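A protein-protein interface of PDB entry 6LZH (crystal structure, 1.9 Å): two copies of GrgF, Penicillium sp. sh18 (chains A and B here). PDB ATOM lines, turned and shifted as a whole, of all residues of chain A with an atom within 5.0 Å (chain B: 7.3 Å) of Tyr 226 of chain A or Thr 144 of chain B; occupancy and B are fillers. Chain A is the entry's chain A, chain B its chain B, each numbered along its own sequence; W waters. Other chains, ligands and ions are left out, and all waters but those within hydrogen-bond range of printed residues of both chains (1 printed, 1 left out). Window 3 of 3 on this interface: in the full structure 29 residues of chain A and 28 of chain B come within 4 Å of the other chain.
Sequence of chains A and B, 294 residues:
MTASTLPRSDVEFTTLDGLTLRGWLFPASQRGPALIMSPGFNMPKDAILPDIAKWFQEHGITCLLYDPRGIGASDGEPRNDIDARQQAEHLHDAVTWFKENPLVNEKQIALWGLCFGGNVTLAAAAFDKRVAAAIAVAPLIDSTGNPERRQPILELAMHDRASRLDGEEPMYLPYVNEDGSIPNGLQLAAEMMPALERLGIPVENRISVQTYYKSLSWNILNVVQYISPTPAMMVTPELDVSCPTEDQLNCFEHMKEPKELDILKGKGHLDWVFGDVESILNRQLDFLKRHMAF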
ATOM      1  N   ALA A 125     -26.670  -7.876  -4.885  1.00  0.00           N
ATOM      2  CA  ALA A 125     -27.839  -8.356  -4.148  1.00  0.00           C
ATOM      3  C   ALA A 125     -27.899  -7.757  -2.749  1.00  0.00           C
ATOM      4  O   ALA A 125     -28.983  -7.648  -2.163  1.00  0.00           O
ATOM      5  CB  ALA A 125     -27.812  -9.881  -4.049  1.00  0.00           C
ATOM      6  N   ALA A 126     -26.749  -7.382  -2.196  1.00  0.00           N
ATOM      7  CA  ALA A 126     -26.736  -6.755  -0.875  1.00  0.00           C
ATOM      8  C   ALA A 126     -27.453  -5.413  -0.895  1.00  0.00           C
ATOM      9  O   ALA A 126     -28.016  -4.992   0.121  1.00  0.00           O
ATOM     10  CB  ALA A 126     -25.288  -6.571  -0.403  1.00  0.00           C
ATOM     11  N   PHE A 127     -27.428  -4.719  -2.031  1.00  0.00           N
ATOM     12  CA  PHE A 127     -27.886  -3.338  -2.086  1.00  0.00           C
ATOM     13  C   PHE A 127     -29.213  -3.156  -2.810  1.00  0.00           C
ATOM     14  O   PHE A 127     -29.913  -2.166  -2.543  1.00  0.00           O
ATOM     15  CB  PHE A 127     -26.825  -2.461  -2.779  1.00  0.00           C
ATOM     16  CG  PHE A 127     -25.474  -2.506  -2.123  1.00  0.00           C
ATOM     17  CD1 PHE A 127     -25.359  -2.425  -0.741  1.00  0.00           C
ATOM     18  CD2 PHE A 127     -24.316  -2.620  -2.885  1.00  0.00           C
ATOM     19  CE1 PHE A 127     -24.106  -2.467  -0.118  1.00  0.00           C
ATOM     20  CE2 PHE A 127     -23.068  -2.646  -2.273  1.00  0.00           C
ATOM     21  CZ  PHE A 127     -22.971  -2.575  -0.877  1.00  0.00           C
ATOM     22  N   LYS A 129     -32.838  -4.358  -3.629  1.00  0.00           N
ATOM     23  CA  LYS A 129     -33.973  -5.223  -3.309  1.00  0.00           C
ATOM     24  C   LYS A 129     -34.941  -5.413  -4.476  1.00  0.00           C
ATOM     25  O   LYS A 129     -35.950  -6.106  -4.304  1.00  0.00           O
ATOM     26  CB  LYS A 129     -34.719  -4.666  -2.084  1.00  0.00           C
ATOM     27  CG  LYS A 129     -33.872  -4.687  -0.837  1.00  0.00           C
ATOM     28  CD  LYS A 129     -33.425  -6.103  -0.516  1.00  0.00           C
ATOM     29  CE  LYS A 129     -32.167  -6.087   0.335  1.00  0.00           C
ATOM     30  NZ  LYS A 129     -31.038  -6.829  -0.279  1.00  0.00           N
ATOM     31  N   ASN A 222     -17.993  -7.745   4.315  1.00  0.00           N
ATOM     32  CA  ASN A 222     -18.579  -6.635   5.059  1.00  0.00           C
ATOM     33  C   ASN A 222     -19.991  -6.270   4.616  1.00  0.00           C
ATOM     34  O   ASN A 222     -20.640  -5.465   5.297  1.00  0.00           O
ATOM     35  CB  ASN A 222     -17.698  -5.400   4.931  1.00  0.00           C
ATOM     36  CG  ASN A 222     -16.496  -5.433   5.867  1.00  0.00           C
ATOM     37  OD1 ASN A 222     -15.804  -4.432   6.026  1.00  0.00           O
ATOM     38  ND2 ASN A 222     -16.250  -6.582   6.489  1.00  0.00           N
ATOM     39  N   VAL A 223     -20.483  -6.798   3.486  1.00  0.00           N
ATOM     40  CA  VAL A 223     -21.808  -6.386   3.034  1.00  0.00           C
ATOM     41  C   VAL A 223     -22.738  -7.568   2.773  1.00  0.00           C
ATOM     42  O   VAL A 223     -23.943  -7.366   2.585  1.00  0.00           O
ATOM     43  CB  VAL A 223     -21.718  -5.477   1.787  1.00  0.00           C
ATOM     44  CG1 VAL A 223     -20.694  -4.344   2.009  1.00  0.00           C
ATOM     45  CG2 VAL A 223     -21.385  -6.275   0.527  1.00  0.00           C
ATOM     46  N   VAL A 224     -22.219  -8.803   2.767  1.00  0.00           N
ATOM     47  CA  VAL A 224     -23.097  -9.925   2.414  1.00  0.00           C
ATOM     48  C   VAL A 224     -24.176 -10.171   3.469  1.00  0.00           C
ATOM     49  O   VAL A 224     -25.221 -10.771   3.162  1.00  0.00           O
ATOM     50  CB  VAL A 224     -22.303 -11.216   2.151  1.00  0.00           C
ATOM     51  CG1 VAL A 224     -21.505 -11.084   0.867  1.00  0.00           C
ATOM     52  CG2 VAL A 224     -21.410 -11.591   3.360  1.00  0.00           C
ATOM     53  N   GLN A 225     -23.982  -9.687   4.702  1.00  0.00           N
ATOM     54  CA  GLN A 225     -25.040  -9.816   5.700  1.00  0.00           C
ATOM     55  C   GLN A 225     -26.282  -9.019   5.326  1.00  0.00           C
ATOM     56  O   GLN A 225     -27.364  -9.302   5.856  1.00  0.00           O
ATOM     57  CB  GLN A 225     -24.534  -9.388   7.085  1.00  0.00           C
ATOM     58  CG  GLN A 225     -24.294  -7.907   7.230  1.00  0.00           C
ATOM     59  CD  GLN A 225     -22.844  -7.526   6.962  1.00  0.00           C
ATOM     60  OE1 GLN A 225     -22.158  -8.161   6.143  1.00  0.00           O
ATOM     61  NE2 GLN A 225     -22.359  -6.500   7.674  1.00  0.00           N
ATOM     62  N   TYR A 226     -26.163  -8.060   4.406  1.00  0.00           N
ATOM     63  CA  TYR A 226     -27.300  -7.253   3.972  1.00  0.00           C
ATOM     64  C   TYR A 226     -28.088  -7.871   2.828  1.00  0.00           C
ATOM     65  O   TYR A 226     -29.101  -7.300   2.404  1.00  0.00           O
ATOM     66  CB  TYR A 226     -26.836  -5.862   3.549  1.00  0.00           C
ATOM     67  CG  TYR A 226     -26.056  -5.107   4.615  1.00  0.00           C
ATOM     68  CD1 TYR A 226     -26.553  -4.965   5.903  1.00  0.00           C
ATOM     69  CD2 TYR A 226     -24.837  -4.535   4.320  1.00  0.00           C
ATOM     70  CE1 TYR A 226     -25.860  -4.264   6.867  1.00  0.00           C
ATOM     71  CE2 TYR A 226     -24.125  -3.834   5.281  1.00  0.00           C
ATOM     72  CZ  TYR A 226     -24.642  -3.701   6.555  1.00  0.00           C
ATOM     73  OH  TYR A 226     -23.930  -3.002   7.512  1.00  0.00           O
ATOM     74  N   ILE A 227     -27.649  -8.999   2.280  1.00  0.00           N
ATOM     75  CA  ILE A 227     -28.424  -9.597   1.201  1.00  0.00           C
ATOM     76  C   ILE A 227     -29.813  -9.975   1.701  1.00  0.00           C
ATOM     77  O   ILE A 227     -30.826  -9.649   1.075  1.00  0.00           O
ATOM     78  CB  ILE A 227     -27.671 -10.799   0.609  1.00  0.00           C
ATOM     79  CG1 ILE A 227     -26.351 -10.338  -0.027  1.00  0.00           C
ATOM     80  CG2 ILE A 227     -28.571 -11.547  -0.390  1.00  0.00           C
ATOM     81  CD1 ILE A 227     -25.389 -11.477  -0.333  1.00  0.00           C
ATOM     82  N   SER A 228     -29.885 -10.638   2.848  1.00  0.00           N
ATOM     83  CA  SER A 228     -31.188 -11.076   3.332  1.00  0.00           C
ATOM     84  C   SER A 228     -32.091  -9.856   3.534  1.00  0.00           C
ATOM     85  O   SER A 228     -31.641  -8.829   4.055  1.00  0.00           O
ATOM     86  CB  SER A 228     -31.060 -11.862   4.636  1.00  0.00           C
ATOM     87  OG  SER A 228     -32.321 -12.016   5.272  1.00  0.00           O
ATOM     88  N   LEU B 140     -14.298  10.217  11.965  1.00  0.00           N
ATOM     89  CA  LEU B 140     -15.578   9.526  11.856  1.00  0.00           C
ATOM     90  C   LEU B 140     -15.308   8.111  11.369  1.00  0.00           C
ATOM     91  O   LEU B 140     -14.803   7.922  10.254  1.00  0.00           O
ATOM     92  CB  LEU B 140     -16.508  10.273  10.896  1.00  0.00           C
ATOM     93  CG  LEU B 140     -17.830   9.598  10.496  1.00  0.00           C
ATOM     94  CD1 LEU B 140     -18.530   8.982  11.694  1.00  0.00           C
ATOM     95  CD2 LEU B 140     -18.744  10.608   9.812  1.00  0.00           C
ATOM     96  N   ILE B 141     -15.631   7.124  12.197  1.00  0.00           N
ATOM     97  CA  ILE B 141     -15.252   5.752  11.895  1.00  0.00           C
ATOM     98  C   ILE B 141     -16.368   4.999  11.175  1.00  0.00           C
ATOM     99  O   ILE B 141     -16.109   4.256  10.229  1.00  0.00           O
ATOM    100  CB  ILE B 141     -14.825   5.035  13.189  1.00  0.00           C
ATOM    101  CG1 ILE B 141     -13.716   5.807  13.910  1.00  0.00           C
ATOM    102  CG2 ILE B 141     -14.345   3.641  12.872  1.00  0.00           C
ATOM    103  CD1 ILE B 141     -12.431   5.980  13.101  1.00  0.00           C
ATOM    104  N   ASP B 142     -17.619   5.150  11.595  1.00  0.00           N
ATOM    105  CA  ASP B 142     -18.694   4.358  11.008  1.00  0.00           C
ATOM    106  C   ASP B 142     -19.953   5.199  10.881  1.00  0.00           C
ATOM    107  O   ASP B 142     -20.356   5.856  11.843  1.00  0.00           O
ATOM    108  CB  ASP B 142     -18.973   3.102  11.850  1.00  0.00           C
ATOM    109  CG  ASP B 142     -20.176   2.316  11.350  1.00  0.00           C
ATOM    110  OD1 ASP B 142     -20.337   2.175  10.112  1.00  0.00           O
ATOM    111  OD2 ASP B 142     -20.959   1.847  12.203  1.00  0.00           O
ATOM    112  N   SER B 143     -20.564   5.179   9.690  1.00  0.00           N
ATOM    113  CA  SER B 143     -21.792   5.912   9.391  1.00  0.00           C
ATOM    114  C   SER B 143     -22.975   4.983   9.141  1.00  0.00           C
ATOM    115  O   SER B 143     -23.984   5.410   8.571  1.00  0.00           O
ATOM    116  CB  SER B 143     -21.597   6.814   8.170  1.00  0.00           C
ATOM    117  OG  SER B 143     -21.035   8.062   8.526  1.00  0.00           O
ATOM    118  N   THR B 144     -22.863   3.710   9.530  1.00  0.00           N
ATOM    119  CA  THR B 144     -23.929   2.758   9.231  1.00  0.00           C
ATOM    120  C   THR B 144     -25.221   3.118   9.955  1.00  0.00           C
ATOM    121  O   THR B 144     -26.318   2.923   9.409  1.00  0.00           O
ATOM    122  CB  THR B 144     -23.477   1.346   9.601  1.00  0.00           C
ATOM    123  OG1 THR B 144     -22.327   0.999   8.816  1.00  0.00           O
ATOM    124  CG2 THR B 144     -24.597   0.334   9.357  1.00  0.00           C
ATOM    125  N   GLY B 145     -25.114   3.680  11.158  1.00  0.00           N
ATOM    126  CA  GLY B 145     -26.308   3.941  11.938  1.00  0.00           C
ATOM    127  C   GLY B 145     -26.961   2.633  12.333  1.00  0.00           C
ATOM    128  O   GLY B 145     -26.289   1.625  12.587  1.00  0.00           O
ATOM    129  N   ASN B 146     -28.286   2.641  12.387  1.00  0.00           N
ATOM    130  CA  ASN B 146     -29.025   1.410  12.626  1.00  0.00           C
ATOM    131  C   ASN B 146     -29.071   0.622  11.323  1.00  0.00           C
ATOM    132  O   ASN B 146     -29.724   1.057  10.365  1.00  0.00           O
ATOM    133  CB  ASN B 146     -30.438   1.720  13.135  1.00  0.00           C
ATOM    134  CG  ASN B 146     -31.227   0.469  13.486  1.00  0.00           C
ATOM    135  OD1 ASN B 146     -30.839  -0.648  13.144  1.00  0.00           O
ATOM    136  ND2 ASN B 146     -32.353   0.655  14.169  1.00  0.00           N
ATOM    137  N   PRO B 147     -28.394  -0.529  11.241  1.00  0.00           N
ATOM    138  CA  PRO B 147     -28.398  -1.289   9.980  1.00  0.00           C
ATOM    139  C   PRO B 147     -29.769  -1.801   9.600  1.00  0.00           C
ATOM    140  O   PRO B 147     -30.002  -2.060   8.413  1.00  0.00           O
ATOM    141  CB  PRO B 147     -27.423  -2.446  10.253  1.00  0.00           C
ATOM    142  CG  PRO B 147     -26.621  -2.006  11.453  1.00  0.00           C
ATOM    143  CD  PRO B 147     -27.586  -1.199  12.272  1.00  0.00           C
ATOM    144  N   GLU B 148     -30.679  -1.955  10.566  1.00  0.00           N
ATOM    145  CA  GLU B 148     -32.074  -2.278  10.291  1.00  0.00           C
ATOM    146  C   GLU B 148     -32.847  -1.110   9.702  1.00  0.00           C
ATOM    147  O   GLU B 148     -34.033  -1.265   9.407  1.00  0.00           O
ATOM    148  CB  GLU B 148     -32.779  -2.745  11.567  1.00  0.00           C
ATOM    149  CG  GLU B 148     -32.937  -4.244  11.677  1.00  0.00           C
ATOM    150  CD  GLU B 148     -31.610  -4.947  11.789  1.00  0.00           C
ATOM    151  OE1 GLU B 148     -30.752  -4.452  12.546  1.00  0.00           O
ATOM    152  OE2 GLU B 148     -31.421  -5.983  11.117  1.00  0.00           O
ATOM    153  N   ARG B 149     -32.229   0.055   9.552  1.00  0.00           N
ATOM    154  CA  ARG B 149     -32.863   1.211   8.929  1.00  0.00           C
ATOM    155  C   ARG B 149     -32.273   1.485   7.544  1.00  0.00           C
ATOM    156  O   ARG B 149     -32.676   2.442   6.870  1.00  0.00           O
ATOM    157  CB  ARG B 149     -32.733   2.414   9.885  1.00  0.00           C
ATOM    158  CG  ARG B 149     -33.114   3.805   9.392  1.00  0.00           C
ATOM    159  CD  ARG B 149     -34.519   3.968   8.819  1.00  0.00           C
ATOM    160  NE  ARG B 149     -34.518   4.967   7.744  1.00  0.00           N
ATOM    161  CZ  ARG B 149     -34.263   6.264   7.919  1.00  0.00           C
ATOM    162  NH1 ARG B 149     -34.282   7.094   6.882  1.00  0.00           N
ATOM    163  NH2 ARG B 149     -33.992   6.738   9.128  1.00  0.00           N
ATOM    164  N   ARG B 150     -31.363   0.626   7.081  1.00  0.00           N
ATOM    165  CA  ARG B 150     -30.723   0.814   5.785  1.00  0.00           C
ATOM    166  C   ARG B 150     -31.684   0.649   4.613  1.00  0.00           C
ATOM    167  O   ARG B 150     -31.413   1.196   3.540  1.00  0.00           O
ATOM    168  CB  ARG B 150     -29.564  -0.169   5.633  1.00  0.00           C
ATOM    169  CG  ARG B 150     -30.013  -1.570   5.264  1.00  0.00           C
ATOM    170  CD  ARG B 150     -28.887  -2.580   5.396  1.00  0.00           C
ATOM    171  NE  ARG B 150     -29.335  -3.922   5.024  1.00  0.00           N
ATOM    172  CZ  ARG B 150     -29.847  -4.803   5.881  1.00  0.00           C
ATOM    173  NH1 ARG B 150     -30.240  -6.001   5.453  1.00  0.00           N
ATOM    174  NH2 ARG B 150     -29.962  -4.483   7.166  1.00  0.00           N
ATOM    175  N   ILE B 153     -33.274   3.800   2.744  1.00  0.00           N
ATOM    176  CA  ILE B 153     -32.262   4.588   2.051  1.00  0.00           C
ATOM    177  C   ILE B 153     -31.751   3.842   0.825  1.00  0.00           C
ATOM    178  O   ILE B 153     -31.596   4.430  -0.249  1.00  0.00           O
ATOM    179  CB  ILE B 153     -31.114   4.966   2.998  1.00  0.00           C
ATOM    180  CG1 ILE B 153     -31.652   5.766   4.183  1.00  0.00           C
ATOM    181  CG2 ILE B 153     -30.073   5.786   2.234  1.00  0.00           C
ATOM    182  CD1 ILE B 153     -30.566   6.344   5.061  1.00  0.00           C
ATOM    183  N   LEU B 154     -31.475   2.539   0.962  1.00  0.00           N
ATOM    184  CA  LEU B 154     -30.996   1.780  -0.194  1.00  0.00           C
ATOM    185  C   LEU B 154     -32.035   1.765  -1.309  1.00  0.00           C
ATOM    186  O   LEU B 154     -31.688   1.806  -2.498  1.00  0.00           O
ATOM    187  CB  LEU B 154     -30.628   0.353   0.218  1.00  0.00           C
ATOM    188  CG  LEU B 154     -29.294   0.200   0.965  1.00  0.00           C
ATOM    189  CD1 LEU B 154     -29.115  -1.219   1.519  1.00  0.00           C
ATOM    190  CD2 LEU B 154     -28.112   0.603   0.074  1.00  0.00           C
ATOM    191  N   ASN B 184     -31.013   7.774   8.436  1.00  0.00           N
ATOM    192  CA  ASN B 184     -30.316   6.752   9.216  1.00  0.00           C
ATOM    193  C   ASN B 184     -28.881   7.140   9.554  1.00  0.00           C
ATOM    194  O   ASN B 184     -28.460   7.048  10.713  1.00  0.00           O
ATOM    195  CB  ASN B 184     -30.322   5.416   8.476  1.00  0.00           C
ATOM    196  CG  ASN B 184     -29.771   4.286   9.333  1.00  0.00           C
ATOM    197  OD1 ASN B 184     -29.938   4.288  10.558  1.00  0.00           O
ATOM    198  ND2 ASN B 184     -29.106   3.325   8.700  1.00  0.00           N
ATOM    199  N   GLY B 185     -28.097   7.523   8.559  1.00  0.00           N
ATOM    200  CA  GLY B 185     -26.702   7.799   8.849  1.00  0.00           C
ATOM    201  C   GLY B 185     -26.400   9.274   9.010  1.00  0.00           C
ATOM    202  O   GLY B 185     -25.289   9.718   8.701  1.00  0.00           O
ATOM    203  N   LEU B 186     -27.373  10.041   9.510  1.00  0.00           N
ATOM    204  CA  LEU B 186     -27.295  11.499   9.515  1.00  0.00           C
ATOM    205  C   LEU B 186     -27.365  12.092  10.919  1.00  0.00           C
ATOM    206  O   LEU B 186     -27.721  13.265  11.075  1.00  0.00           O
ATOM    207  CB  LEU B 186     -28.395  12.094   8.635  1.00  0.00           C
ATOM    208  CG  LEU B 186     -28.288  11.809   7.131  1.00  0.00           C
ATOM    209  CD1 LEU B 186     -29.177  12.746   6.316  1.00  0.00           C
ATOM    210  CD2 LEU B 186     -26.836  11.886   6.655  1.00  0.00           C
ATOM    211  N   TYR B 212     -24.989   7.229   1.386  1.00  0.00           N
ATOM    212  CA  TYR B 212     -25.146   6.057   2.242  1.00  0.00           C
ATOM    213  C   TYR B 212     -24.807   4.766   1.492  1.00  0.00           C
ATOM    214  O   TYR B 212     -24.238   3.835   2.072  1.00  0.00           O
ATOM    215  CB  TYR B 212     -26.567   6.013   2.797  1.00  0.00           C
ATOM    216  CG  TYR B 212     -26.781   4.992   3.892  1.00  0.00           C
ATOM    217  CD1 TYR B 212     -26.401   5.257   5.206  1.00  0.00           C
ATOM    218  CD2 TYR B 212     -27.373   3.761   3.616  1.00  0.00           C
ATOM    219  CE1 TYR B 212     -26.604   4.321   6.213  1.00  0.00           C
ATOM    220  CE2 TYR B 212     -27.576   2.821   4.610  1.00  0.00           C
ATOM    221  CZ  TYR B 212     -27.201   3.103   5.904  1.00  0.00           C
ATOM    222  OH  TYR B 212     -27.414   2.158   6.885  1.00  0.00           O
ATOM    223  N   SER B 215     -21.015   4.291   1.379  1.00  0.00           N
ATOM    224  CA  SER B 215     -20.392   4.122   2.678  1.00  0.00           C
ATOM    225  C   SER B 215     -20.509   2.696   3.195  1.00  0.00           C
ATOM    226  O   SER B 215     -19.656   2.268   3.980  1.00  0.00           O
ATOM    227  CB  SER B 215     -20.994   5.115   3.678  1.00  0.00           C
ATOM    228  OG  SER B 215     -22.118   4.562   4.351  1.00  0.00           O
ATOM    229  N   LEU B 216     -21.520   1.936   2.760  1.00  0.00           N
ATOM    230  CA  LEU B 216     -21.650   0.577   3.270  1.00  0.00           C
ATOM    231  C   LEU B 216     -20.534  -0.319   2.757  1.00  0.00           C
ATOM    232  O   LEU B 216     -20.191  -1.308   3.414  1.00  0.00           O
ATOM    233  CB  LEU B 216     -23.021  -0.011   2.906  1.00  0.00           C
ATOM    234  CG  LEU B 216     -24.246   0.532   3.663  1.00  0.00           C
ATOM    235  CD1 LEU B 216     -25.501  -0.241   3.264  1.00  0.00           C
ATOM    236  CD2 LEU B 216     -24.063   0.502   5.176  1.00  0.00           C
ATOM    237  N   SER B 217     -19.956  -0.001   1.600  1.00  0.00           N
ATOM    238  CA  SER B 217     -18.806  -0.741   1.110  1.00  0.00           C
ATOM    239  C   SER B 217     -17.482  -0.113   1.547  1.00  0.00           C
ATOM    240  O   SER B 217     -16.421  -0.531   1.065  1.00  0.00           O
ATOM    241  CB  SER B 217     -18.882  -0.889  -0.419  1.00  0.00           C
ATOM    242  OG  SER B 217     -18.596   0.317  -1.114  1.00  0.00           O
ATOM    243  N   TRP B 218     -17.525   0.845   2.479  1.00  0.00           N
ATOM    244  CA  TRP B 218     -16.342   1.522   3.011  1.00  0.00           C
ATOM    245  C   TRP B 218     -16.222   1.257   4.504  1.00  0.00           C
ATOM    246  O   TRP B 218     -17.088   1.662   5.283  1.00  0.00           O
ATOM    247  CB  TRP B 218     -16.417   3.030   2.773  1.00  0.00           C
ATOM    248  CG  TRP B 218     -15.157   3.739   3.158  1.00  0.00           C
ATOM    249  CD1 TRP B 218     -14.947   4.505   4.274  1.00  0.00           C
ATOM    250  CD2 TRP B 218     -13.920   3.726   2.432  1.00  0.00           C
ATOM    251  NE1 TRP B 218     -13.655   5.001   4.266  1.00  0.00           N
ATOM    252  CE2 TRP B 218     -13.006   4.528   3.150  1.00  0.00           C
ATOM    253  CE3 TRP B 218     -13.503   3.136   1.226  1.00  0.00           C
ATOM    254  CZ2 TRP B 218     -11.702   4.747   2.706  1.00  0.00           C
ATOM    255  CZ3 TRP B 218     -12.197   3.344   0.792  1.00  0.00           C
ATOM    256  CH2 TRP B 218     -11.314   4.150   1.529  1.00  0.00           C
HETATM  257  O   HOH W   1     -29.965  -8.400   6.135  1.00  0.00           O
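The backbone carbonyl oxygen (O) of Ser 228 of chain A sits at hydrogen-bond distance from the guanidinium group (NH1) of Arg 150 of chain B.
O of Thr 144 of chain B is in hydrogen-bond range of ND2 of Asn 184 of chain B (2.9 Å). The backbone carbonyl oxygen of Pro 147 of chain B sits at hydrogen-bond distance from the guanidinium group of Arg 150 of chain B, at 2.7 Å. The side-chain carboxylate of Asp 142 of chain B sits at hydrogen-bond distance from the side-chain hydroxyl of Thr 144 of chain B, 2.7 Å away. The side-chain amino group (NZ) of Lys 129 of chain A lies within hydrogen-bond range of the backbone carbonyl oxygen (O) of Tyr 226 of chain A (3.3 Å). The backbone carbonyl oxygen (O) of Thr 144 of chain B sits at hydrogen-bond distance from the side-chain hydroxyl (OH) of Tyr 212 of chain B. The backbone NH (N) of Val 223 of chain A lies within hydrogen-bond range of the side-chain amide oxygen (OE1) of Gln 225 of chain A (3.4 Å).
Among the printed residues, merely in contact across the chains: Tyr 226 of chain A with Arg 150 of chain B (3.1 Å), Val 223 of chain A with Leu 216 of chain B (3.4 Å), Phe 127 of chain A with Leu 154 of chain B (3.8 Å) and Tyr 226 of chain A with Thr 144 of chain B (3.9 Å).
Of the printed residues of chain B, Tyr 226 of chain A touches Thr 144 and Arg 150. Of the printed residues of chain B, Ser 228 of chain A touches Arg 150. Printed residues of chain A within 4 Å of Thr 144 of chain B: Tyr 226. Of the printed residues of chain A, Arg 150 of chain B touches Tyr 226 (3.1 Å) and Ser 228 (3.5 Å). Tyr 212 of chain B touches none of the printed residues of chain A. Ser 215 of chain B touches none of the printed residues of chain A. Printed residues of chain A within 4 Å of Leu 216 of chain B: Val 223 (3.4 Å). The nearest residue of chain B that does not touch Tyr 226 of chain A is Pro 147 of chain B (4.1 Å). The nearest printed residue of chain A that does not touch Thr 144 of chain B is Gln 225 of chain A (7.4 Å). The nearest printed residue of chain A that does not touch Leu 154 of chain B is Ala 126 of chain A (4.2 Å).
Of the 21 printed residues of chain B, 4 touch a printed residue of chain A.
No position is printed for both chains. Of the 5 pairs that touch across the chains among the printed residues, none has its exchanged pair printed and touching as well.
Water W1 lies within hydrogen-bond range of the guanidinium group of Arg 150 of chain B (2.5 Å), the backbone carbonyl oxygen of Ser 228 of chain A (2.7 Å) and the backbone carbonyl oxygen of Gln 225 of chain A (2.8 Å).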
